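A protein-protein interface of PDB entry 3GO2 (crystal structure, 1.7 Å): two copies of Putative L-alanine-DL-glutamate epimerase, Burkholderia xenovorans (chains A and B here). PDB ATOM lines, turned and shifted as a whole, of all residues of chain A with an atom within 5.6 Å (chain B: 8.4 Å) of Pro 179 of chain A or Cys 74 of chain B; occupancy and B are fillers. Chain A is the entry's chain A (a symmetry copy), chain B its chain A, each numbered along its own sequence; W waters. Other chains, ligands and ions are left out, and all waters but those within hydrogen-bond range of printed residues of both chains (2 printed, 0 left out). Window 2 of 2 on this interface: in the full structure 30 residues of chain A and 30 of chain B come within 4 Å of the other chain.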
ATOM      1  N   TRP A 177      35.612   9.829  24.738  1.00  0.00           N
ATOM      2  CA  TRP A 177      34.745  10.945  24.412  1.00  0.00           C
ATOM      3  C   TRP A 177      35.011  11.256  22.948  1.00  0.00           C
ATOM      4  O   TRP A 177      36.040  11.865  22.616  1.00  0.00           O
ATOM      5  CB  TRP A 177      35.055  12.155  25.301  1.00  0.00           C
ATOM      6  CG  TRP A 177      34.154  13.368  25.038  1.00  0.00           C
ATOM      7  CD1 TRP A 177      34.504  14.554  24.401  1.00  0.00           C
ATOM      8  CD2 TRP A 177      32.782  13.496  25.385  1.00  0.00           C
ATOM      9  NE1 TRP A 177      33.422  15.380  24.354  1.00  0.00           N
ATOM     10  CE2 TRP A 177      32.355  14.767  24.940  1.00  0.00           C
ATOM     11  CE3 TRP A 177      31.860  12.650  25.993  1.00  0.00           C
ATOM     12  CZ2 TRP A 177      31.049  15.219  25.107  1.00  0.00           C
ATOM     13  CZ3 TRP A 177      30.555  13.102  26.171  1.00  0.00           C
ATOM     14  CH2 TRP A 177      30.165  14.379  25.722  1.00  0.00           C
ATOM     15  N   ARG A 178      34.080  10.840  22.081  1.00  0.00           N
ATOM     16  CA  ARG A 178      34.235  10.932  20.619  1.00  0.00           C
ATOM     17  C   ARG A 178      32.940  11.432  19.967  1.00  0.00           C
ATOM     18  O   ARG A 178      32.462  10.861  18.972  1.00  0.00           O
ATOM     19  CB  ARG A 178      34.604   9.577  20.012  1.00  0.00           C
ATOM     20  CG  ARG A 178      35.866   8.956  20.572  1.00  0.00           C
ATOM     21  CD  ARG A 178      35.890   7.483  20.318  1.00  0.00           C
ATOM     22  NE  ARG A 178      35.792   7.241  18.896  1.00  0.00           N
ATOM     23  CZ  ARG A 178      35.223   6.183  18.335  1.00  0.00           C
ATOM     24  NH1 ARG A 178      35.181   6.103  17.001  1.00  0.00           N
ATOM     25  NH2 ARG A 178      34.696   5.210  19.075  1.00  0.00           N
ATOM     26  N   PRO A 179      32.376  12.529  20.505  1.00  0.00           N
ATOM     27  CA  PRO A 179      31.113  13.019  19.936  1.00  0.00           C
ATOM     28  C   PRO A 179      31.201  13.375  18.439  1.00  0.00           C
ATOM     29  O   PRO A 179      30.202  13.308  17.718  1.00  0.00           O
ATOM     30  CB  PRO A 179      30.811  14.267  20.777  1.00  0.00           C
ATOM     31  CG  PRO A 179      32.124  14.759  21.191  1.00  0.00           C
ATOM     32  CD  PRO A 179      32.937  13.481  21.465  1.00  0.00           C
ATOM     33  N   GLY A 180      32.363  13.781  17.960  1.00  0.00           N
ATOM     34  CA  GLY A 180      32.496  14.068  16.534  1.00  0.00           C
ATOM     35  C   GLY A 180      32.220  12.869  15.647  1.00  0.00           C
ATOM     36  O   GLY A 180      31.874  13.031  14.470  1.00  0.00           O
ATOM     37  N   PHE A 181      32.381  11.670  16.218  1.00  0.00           N
ATOM     38  CA  PHE A 181      32.043  10.416  15.538  1.00  0.00           C
ATOM     39  C   PHE A 181      30.821   9.723  16.159  1.00  0.00           C
ATOM     40  O   PHE A 181      30.617   8.499  15.954  1.00  0.00           O
ATOM     41  CB  PHE A 181      33.247   9.463  15.532  1.00  0.00           C
ATOM     42  CG  PHE A 181      34.500  10.014  14.900  1.00  0.00           C
ATOM     43  CD1 PHE A 181      34.469  10.849  13.789  1.00  0.00           C
ATOM     44  CD2 PHE A 181      35.746   9.605  15.360  1.00  0.00           C
ATOM     45  CE1 PHE A 181      35.633  11.315  13.206  1.00  0.00           C
ATOM     46  CE2 PHE A 181      36.907  10.069  14.767  1.00  0.00           C
ATOM     47  CZ  PHE A 181      36.850  10.910  13.692  1.00  0.00           C
ATOM     48  N   ALA A 182      29.998  10.529  16.857  1.00  0.00           N
ATOM     49  CA  ALA A 182      28.703  10.139  17.435  1.00  0.00           C
ATOM     50  C   ALA A 182      28.819   9.084  18.527  1.00  0.00           C
ATOM     51  O   ALA A 182      27.895   8.282  18.725  1.00  0.00           O
ATOM     52  CB  ALA A 182      27.724   9.705  16.342  1.00  0.00           C
ATOM     53  N   VAL A 183      29.941   9.097  19.244  1.00  0.00           N
ATOM     54  CA  VAL A 183      30.081   8.312  20.463  1.00  0.00           C
ATOM     55  C   VAL A 183      30.558   9.238  21.583  1.00  0.00           C
ATOM     56  O   VAL A 183      31.755   9.433  21.761  1.00  0.00           O
ATOM     57  CB  VAL A 183      31.025   7.116  20.283  1.00  0.00           C
ATOM     58  CG1 VAL A 183      31.062   6.310  21.575  1.00  0.00           C
ATOM     59  CG2 VAL A 183      30.560   6.239  19.124  1.00  0.00           C
ATOM     60  N   PRO A 184      29.622   9.838  22.321  1.00  0.00           N
ATOM     61  CA  PRO A 184      28.145   9.701  22.227  1.00  0.00           C
ATOM     62  C   PRO A 184      27.541  10.616  21.158  1.00  0.00           C
ATOM     63  O   PRO A 184      28.232  11.486  20.641  1.00  0.00           O
ATOM     64  CB  PRO A 184      27.704  10.182  23.589  1.00  0.00           C
ATOM     65  CG  PRO A 184      28.633  11.273  23.884  1.00  0.00           C
ATOM     66  CD  PRO A 184      29.976  10.846  23.330  1.00  0.00           C
ATOM     67  N   PHE A 185      26.256  10.434  20.858  1.00  0.00           N
ATOM     68  CA  PHE A 185      25.591  11.313  19.911  1.00  0.00           C
ATOM     69  C   PHE A 185      25.225  12.578  20.652  1.00  0.00           C
ATOM     70  O   PHE A 185      24.284  12.606  21.476  1.00  0.00           O
ATOM     71  CB  PHE A 185      24.349  10.675  19.308  1.00  0.00           C
ATOM     72  CG  PHE A 185      23.639  11.572  18.322  1.00  0.00           C
ATOM     73  CD1 PHE A 185      24.187  11.805  17.070  1.00  0.00           C
ATOM     74  CD2 PHE A 185      22.458  12.200  18.655  1.00  0.00           C
ATOM     75  CE1 PHE A 185      23.566  12.630  16.173  1.00  0.00           C
ATOM     76  CE2 PHE A 185      21.820  13.041  17.735  1.00  0.00           C
ATOM     77  CZ  PHE A 185      22.383  13.232  16.492  1.00  0.00           C
ATOM     78  N   GLN A 186      25.989  13.629  20.390  1.00  0.00           N
ATOM     79  CA  GLN A 186      25.786  14.944  20.978  1.00  0.00           C
ATOM     80  C   GLN A 186      26.361  15.933  19.955  1.00  0.00           C
ATOM     81  O   GLN A 186      27.478  16.442  20.083  1.00  0.00           O
ATOM     82  CB  GLN A 186      26.498  15.043  22.327  1.00  0.00           C
ATOM     83  CG  GLN A 186      26.166  16.285  23.087  1.00  0.00           C
ATOM     84  CD  GLN A 186      26.922  16.344  24.393  1.00  0.00           C
ATOM     85  OE1 GLN A 186      27.876  17.112  24.534  1.00  0.00           O
ATOM     86  NE2 GLN A 186      26.534  15.488  25.344  1.00  0.00           N
ATOM     87  N   PRO A 187      25.597  16.158  18.886  1.00  0.00           N
ATOM     88  CA  PRO A 187      26.180  16.695  17.672  1.00  0.00           C
ATOM     89  C   PRO A 187      26.659  18.144  17.711  1.00  0.00           C
ATOM     90  O   PRO A 187      27.372  18.583  16.789  1.00  0.00           O
ATOM     91  CB  PRO A 187      25.059  16.501  16.647  1.00  0.00           C
ATOM     92  CG  PRO A 187      23.795  16.518  17.454  1.00  0.00           C
ATOM     93  CD  PRO A 187      24.163  15.827  18.724  1.00  0.00           C
ATOM     94  N   LEU A 189      28.838  19.152  19.747  1.00  0.00           N
ATOM     95  CA  LEU A 189      30.246  19.001  20.103  1.00  0.00           C
ATOM     96  C   LEU A 189      30.698  20.060  21.118  1.00  0.00           C
ATOM     97  O   LEU A 189      31.837  20.517  21.096  1.00  0.00           O
ATOM     98  CB  LEU A 189      31.146  19.042  18.850  1.00  0.00           C
ATOM     99  CG  LEU A 189      30.679  18.239  17.639  1.00  0.00           C
ATOM    100  CD1 LEU A 189      31.718  18.324  16.503  1.00  0.00           C
ATOM    101  CD2 LEU A 189      30.390  16.749  17.985  1.00  0.00           C
ATOM    102  N   PHE A 222      37.784  15.374  15.477  1.00  0.00           N
ATOM    103  CA  PHE A 222      36.785  16.371  15.113  1.00  0.00           C
ATOM    104  C   PHE A 222      35.833  16.637  16.294  1.00  0.00           C
ATOM    105  O   PHE A 222      34.663  16.935  16.082  1.00  0.00           O
ATOM    106  CB  PHE A 222      35.909  15.870  13.952  1.00  0.00           C
ATOM    107  CG  PHE A 222      36.587  15.748  12.589  1.00  0.00           C
ATOM    108  CD1 PHE A 222      36.466  16.771  11.637  1.00  0.00           C
ATOM    109  CD2 PHE A 222      37.185  14.558  12.198  1.00  0.00           C
ATOM    110  CE1 PHE A 222      36.994  16.614  10.355  1.00  0.00           C
ATOM    111  CE2 PHE A 222      37.715  14.411  10.928  1.00  0.00           C
ATOM    112  CZ  PHE A 222      37.603  15.428  10.004  1.00  0.00           C
ATOM    113  N   ASN A 223      36.323  16.490  17.528  1.00  0.00           N
ATOM    114  CA  ASN A 223      35.432  16.420  18.701  1.00  0.00           C
ATOM    115  C   ASN A 223      34.985  17.724  19.329  1.00  0.00           C
ATOM    116  O   ASN A 223      34.297  17.698  20.357  1.00  0.00           O
ATOM    117  CB  ASN A 223      36.068  15.510  19.764  1.00  0.00           C
ATOM    118  CG  ASN A 223      36.116  14.077  19.305  1.00  0.00           C
ATOM    119  OD1 ASN A 223      35.123  13.564  18.769  1.00  0.00           O
ATOM    120  ND2 ASN A 223      37.267  13.423  19.456  1.00  0.00           N
ATOM    121  N   LEU B  53      24.963   2.611   5.723  1.00  0.00           N
ATOM    122  CA  LEU B  53      24.227   3.626   6.473  1.00  0.00           C
ATOM    123  C   LEU B  53      22.782   3.249   6.773  1.00  0.00           C
ATOM    124  O   LEU B  53      22.260   3.568   7.854  1.00  0.00           O
ATOM    125  CB  LEU B  53      24.275   4.978   5.746  1.00  0.00           C
ATOM    126  CG  LEU B  53      25.635   5.652   5.830  1.00  0.00           C
ATOM    127  CD1 LEU B  53      25.640   6.933   4.999  1.00  0.00           C
ATOM    128  CD2 LEU B  53      26.003   5.961   7.298  1.00  0.00           C
ATOM    129  N   ARG B  67      18.171  14.324  12.325  1.00  0.00           N
ATOM    130  CA  ARG B  67      18.917  13.463  13.258  1.00  0.00           C
ATOM    131  C   ARG B  67      19.757  12.440  12.485  1.00  0.00           C
ATOM    132  O   ARG B  67      20.955  12.237  12.775  1.00  0.00           O
ATOM    133  CB  ARG B  67      17.971  12.725  14.211  1.00  0.00           C
ATOM    134  CG  ARG B  67      18.675  11.900  15.289  1.00  0.00           C
ATOM    135  CD  ARG B  67      17.838  10.662  15.654  1.00  0.00           C
ATOM    136  NE  ARG B  67      17.717   9.746  14.521  1.00  0.00           N
ATOM    137  CZ  ARG B  67      18.684   8.963  14.051  1.00  0.00           C
ATOM    138  NH1 ARG B  67      19.884   8.907  14.640  1.00  0.00           N
ATOM    139  NH2 ARG B  67      18.458   8.206  12.992  1.00  0.00           N
ATOM    140  N   PHE B  68      19.135  11.755  11.531  1.00  0.00           N
ATOM    141  CA  PHE B  68      19.875  10.787  10.692  1.00  0.00           C
ATOM    142  C   PHE B  68      21.058  11.489   9.995  1.00  0.00           C
ATOM    143  O   PHE B  68      22.171  10.969   9.958  1.00  0.00           O
ATOM    144  CB  PHE B  68      18.990  10.096   9.649  1.00  0.00           C
ATOM    145  CG  PHE B  68      19.786   9.480   8.513  1.00  0.00           C
ATOM    146  CD1 PHE B  68      20.470   8.306   8.698  1.00  0.00           C
ATOM    147  CD2 PHE B  68      19.938  10.157   7.321  1.00  0.00           C
ATOM    148  CE1 PHE B  68      21.253   7.757   7.686  1.00  0.00           C
ATOM    149  CE2 PHE B  68      20.729   9.620   6.283  1.00  0.00           C
ATOM    150  CZ  PHE B  68      21.386   8.418   6.485  1.00  0.00           C
ATOM    151  N   PHE B  69      20.797  12.648   9.414  1.00  0.00           N
ATOM    152  CA  PHE B  69      21.853  13.351   8.708  1.00  0.00           C
ATOM    153  C   PHE B  69      23.012  13.665   9.654  1.00  0.00           C
ATOM    154  O   PHE B  69      24.188  13.444   9.326  1.00  0.00           O
ATOM    155  CB  PHE B  69      21.338  14.636   8.049  1.00  0.00           C
ATOM    156  CG  PHE B  69      22.422  15.365   7.322  1.00  0.00           C
ATOM    157  CD1 PHE B  69      22.786  14.994   6.035  1.00  0.00           C
ATOM    158  CD2 PHE B  69      23.108  16.379   7.940  1.00  0.00           C
ATOM    159  CE1 PHE B  69      23.830  15.650   5.395  1.00  0.00           C
ATOM    160  CE2 PHE B  69      24.169  17.000   7.316  1.00  0.00           C
ATOM    161  CZ  PHE B  69      24.512  16.644   6.037  1.00  0.00           C
ATOM    162  N   ALA B  70      22.686  14.196  10.839  1.00  0.00           N
ATOM    163  CA  ALA B  70      23.694  14.597  11.793  1.00  0.00           C
ATOM    164  C   ALA B  70      24.509  13.393  12.228  1.00  0.00           C
ATOM    165  O   ALA B  70      25.724  13.455  12.258  1.00  0.00           O
ATOM    166  CB  ALA B  70      23.058  15.295  13.032  1.00  0.00           C
ATOM    167  N   GLU B  71      23.846  12.265  12.458  1.00  0.00           N
ATOM    168  CA  GLU B  71      24.560  11.055  12.893  1.00  0.00           C
ATOM    169  C   GLU B  71      25.436  10.506  11.774  1.00  0.00           C
ATOM    170  O   GLU B  71      26.588  10.101  11.992  1.00  0.00           O
ATOM    171  CB  GLU B  71      23.560   9.997  13.336  1.00  0.00           C
ATOM    172  CG  GLU B  71      24.243   8.725  13.861  1.00  0.00           C
ATOM    173  CD  GLU B  71      23.254   7.662  14.332  1.00  0.00           C
ATOM    174  OE1 GLU B  71      22.172   7.533  13.760  1.00  0.00           O
ATOM    175  OE2 GLU B  71      23.593   6.932  15.268  1.00  0.00           O
ATOM    176  N   ALA B  72      24.884  10.474  10.570  1.00  0.00           N
ATOM    177  CA  ALA B  72      25.606   9.985   9.407  1.00  0.00           C
ATOM    178  C   ALA B  72      26.852  10.815   9.113  1.00  0.00           C
ATOM    179  O   ALA B  72      27.875  10.262   8.775  1.00  0.00           O
ATOM    180  CB  ALA B  72      24.694   9.916   8.171  1.00  0.00           C
ATOM    181  N   TYR B  73      26.736  12.127   9.244  1.00  0.00           N
ATOM    182  CA  TYR B  73      27.863  13.020   9.032  1.00  0.00           C
ATOM    183  C   TYR B  73      28.952  12.704  10.050  1.00  0.00           C
ATOM    184  O   TYR B  73      30.132  12.615   9.687  1.00  0.00           O
ATOM    185  CB  TYR B  73      27.389  14.457   9.168  1.00  0.00           C
ATOM    186  CG  TYR B  73      28.505  15.454   8.912  1.00  0.00           C
ATOM    187  CD1 TYR B  73      29.181  15.476   7.704  1.00  0.00           C
ATOM    188  CD2 TYR B  73      28.878  16.362   9.881  1.00  0.00           C
ATOM    189  CE1 TYR B  73      30.214  16.405   7.462  1.00  0.00           C
ATOM    190  CE2 TYR B  73      29.921  17.272   9.654  1.00  0.00           C
ATOM    191  CZ  TYR B  73      30.568  17.289   8.450  1.00  0.00           C
ATOM    192  OH  TYR B  73      31.561  18.210   8.241  1.00  0.00           O
ATOM    193  N   CYS B  74      28.555  12.485  11.309  1.00  0.00           N
ATOM    194  CA  CYS B  74      29.500  12.097  12.353  1.00  0.00           C
ATOM    195  C   CYS B  74      30.221  10.799  11.982  1.00  0.00           C
ATOM    196  O   CYS B  74      31.452  10.720  12.063  1.00  0.00           O
ATOM    197  CB  CYS B  74      28.809  11.925  13.701  1.00  0.00           C
ATOM    198  SG  CYS B  74      28.250  13.439  14.501  1.00  0.00           S
ATOM    199  N   LEU B  75      29.450   9.790  11.567  1.00  0.00           N
ATOM    200  CA  LEU B  75      29.989   8.461  11.331  1.00  0.00           C
ATOM    201  C   LEU B  75      30.934   8.407  10.148  1.00  0.00           C
ATOM    202  O   LEU B  75      31.802   7.532  10.100  1.00  0.00           O
ATOM    203  CB  LEU B  75      28.859   7.458  11.096  1.00  0.00           C
ATOM    204  CG  LEU B  75      27.930   7.222  12.275  1.00  0.00           C
ATOM    205  CD1 LEU B  75      26.775   6.276  11.840  1.00  0.00           C
ATOM    206  CD2 LEU B  75      28.707   6.692  13.496  1.00  0.00           C
ATOM    207  N   THR B  76      30.767   9.319   9.195  1.00  0.00           N
ATOM    208  CA  THR B  76      31.576   9.322   7.993  1.00  0.00           C
ATOM    209  C   THR B  76      32.403  10.594   7.845  1.00  0.00           C
ATOM    210  O   THR B  76      32.946  10.839   6.768  1.00  0.00           O
ATOM    211  CB  THR B  76      30.703   9.146   6.740  1.00  0.00           C
ATOM    212  OG1 THR B  76      29.726  10.193   6.674  1.00  0.00           O
ATOM    213  CG2 THR B  76      30.020   7.774   6.772  1.00  0.00           C
ATOM    214  N   ARG B  77      32.523  11.374   8.922  1.00  0.00           N
ATOM    215  CA  ARG B  77      33.183  12.690   8.879  1.00  0.00           C
ATOM    216  C   ARG B  77      34.528  12.683   8.136  1.00  0.00           C
ATOM    217  O   ARG B  77      34.774  13.563   7.311  1.00  0.00           O
ATOM    218  CB  ARG B  77      33.339  13.280  10.288  1.00  0.00           C
ATOM    219  CG  ARG B  77      32.870  14.683  10.475  1.00  0.00           C
ATOM    220  CD  ARG B  77      33.114  15.154  11.936  1.00  0.00           C
ATOM    221  NE  ARG B  77      32.424  16.425  12.159  1.00  0.00           N
ATOM    222  CZ  ARG B  77      31.345  16.613  12.883  1.00  0.00           C
ATOM    223  NH1 ARG B  77      30.783  15.629  13.619  1.00  0.00           N
ATOM    224  NH2 ARG B  77      30.837  17.841  12.918  1.00  0.00           N
ATOM    225  N   PRO B  78      35.399  11.687   8.401  1.00  0.00           N
ATOM    226  CA  PRO B  78      36.720  11.734   7.760  1.00  0.00           C
ATOM    227  C   PRO B  78      36.699  11.671   6.235  1.00  0.00           C
ATOM    228  O   PRO B  78      37.541  12.297   5.587  1.00  0.00           O
ATOM    229  CB  PRO B  78      37.437  10.520   8.343  1.00  0.00           C
ATOM    230  CG  PRO B  78      36.776  10.323   9.698  1.00  0.00           C
ATOM    231  CD  PRO B  78      35.329  10.653   9.455  1.00  0.00           C
ATOM    232  N   ALA B  79      35.758  10.923   5.676  1.00  0.00           N
ATOM    233  CA  ALA B  79      35.708  10.739   4.227  1.00  0.00           C
ATOM    234  C   ALA B  79      34.446  11.351   3.655  1.00  0.00           C
ATOM    235  O   ALA B  79      33.909  10.890   2.658  1.00  0.00           O
ATOM    236  CB  ALA B  79      35.812   9.242   3.885  1.00  0.00           C
ATOM    237  N   THR B  80      33.994  12.437   4.274  1.00  0.00           N
ATOM    238  CA  THR B  80      32.804  13.143   3.822  1.00  0.00           C
ATOM    239  C   THR B  80      32.988  13.777   2.445  1.00  0.00           C
ATOM    240  O   THR B  80      34.111  13.971   1.960  1.00  0.00           O
ATOM    241  CB  THR B  80      32.355  14.214   4.861  1.00  0.00           C
ATOM    242  OG1 THR B  80      30.979  14.589   4.635  1.00  0.00           O
ATOM    243  CG2 THR B  80      33.264  15.467   4.814  1.00  0.00           C
ATOM    244  N   ILE B  88      24.327   9.523   1.668  1.00  0.00           N
ATOM    245  CA  ILE B  88      23.571  10.206   2.704  1.00  0.00           C
ATOM    246  C   ILE B  88      22.386  10.981   2.078  1.00  0.00           C
ATOM    247  O   ILE B  88      21.261  10.928   2.583  1.00  0.00           O
ATOM    248  CB  ILE B  88      24.503  11.147   3.496  1.00  0.00           C
ATOM    249  CG1 ILE B  88      25.486  10.306   4.315  1.00  0.00           C
ATOM    250  CG2 ILE B  88      23.684  12.076   4.396  1.00  0.00           C
ATOM    251  CD1 ILE B  88      26.560  11.147   5.021  1.00  0.00           C
HETATM  252  O   HOH W   1      28.392  17.154  14.559  1.00  0.00           O
HETATM  253  O   HOH W   2      27.470  13.519  17.878  1.00  0.00           O
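The side-chain sulfur of Cys 74 of chain B is in hydrogen-bond range of the backbone carbonyl oxygen of Pro 179 of chain A, 3.8 Å away.
The backbone carbonyl oxygen (O) of Gly 180 of chain A lies close to the side-chain sulfur (SG) of Cys 74 of chain B (3.6 Å).
The backbone carbonyl oxygen (O) of Gly 180 of chain A is in hydrogen-bond range of the guanidinium group (NH1) of Arg 77 of chain B, at 2.9 Å.
The side-chain carboxylate (OE1) of Glu 71 of chain B is in salt-bridge range of the guanidinium group (NH1) of Arg 67 of chain B (2.8 Å).
O of Ala 70 of chain B is in hydrogen-bond range of SG of Cys 74 of chain B, at 3.4 Å.
The side-chain sulfur (SG) of Cys 74 of chain B lies within hydrogen-bond range of the guanidinium group (NH1) of Arg 77 of chain B, at 3.5 Å.
N of Gly 180 of chain A sits at hydrogen-bond distance from OD1 of Asn 223 of chain A, 2.9 Å away.
Phe 181 of chain A touches Cys 74 of chain B.
Leu 75 of chain B touches Phe 181 of chain A (CD2 to O, 3.6 Å).
CG of Pro 78 of chain B touches CE1 of Phe 181 of chain A, at 3.8 Å.
Cys 74 of chain B touches Ala 182 of chain A (CB to CB, 3.6 Å).
Phe 185 of chain A touches Glu 71 of chain B (CE1 to N, 3.7 Å).
Leu 189 of chain A touches Arg 77 of chain B.
Arg 77 of chain B touches Phe 222 of chain A.
Pro 179 of chain A touches just one residue of chain B: Cys 74 (3.8 Å).
Of chain A, only Pro 179 (3.8 Å), Gly 180 (3.3 Å), Phe 181 (3.5 Å) and Ala 182 (3.6 Å) come within 4 Å of Cys 74 of chain B.
Printed residues of chain B within 4 Å of Gly 180 of chain A: Cys 74 (3.3 Å) and Arg 77 (2.9 Å).
Of the printed residues of chain A, Leu 75 of chain B touches Phe 181.
Of the printed residues of chain B, Ala 182 of chain A touches Cys 74 (3.6 Å).
Of the printed residues of chain A, Arg 77 of chain B touches Gly 180 (2.9 Å), Leu 189 (3.7 Å) and Phe 222 (3.5 Å).
Of the printed residues of chain A, Glu 71 of chain B touches Phe 185 (3.7 Å).
Ala 72 of chain B touches none of the printed residues of chain A.
Phe 68 of chain B touches none of the printed residues of chain A.
The nearest residue of chain B that does not touch Pro 179 of chain A is Arg 77 of chain B (4.7 Å).
Hydrophobic or aromatic side chains of chain A that line the printed part of chain B: Phe 181, Ala 182, Phe 185, Leu 189 and Phe 222.
Among the printed residues, 10 pairs touch across the chains.
Among the printed residues, no Asp or Glu carboxylate lies within 4 Å of a Lys or Arg side-chain nitrogen of the other chain.
No position is printed for both chains.
Of the 10 pairs that touch across the chains among the printed residues, none has its exchanged pair printed and touching as well.
Water W2 lies within hydrogen-bond range of the backbone carbonyl oxygen of Pro 179 of chain A, the backbone NH of Gln 186 of chain A and the side-chain sulfur of Cys 74 of chain B.
Water W1 lies within hydrogen-bond range of O of Pro 187 of chain A (2.8 Å), NH1 of Arg 77 of chain B (3.0 Å) and SG of Cys 74 of chain B (3.7 Å).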
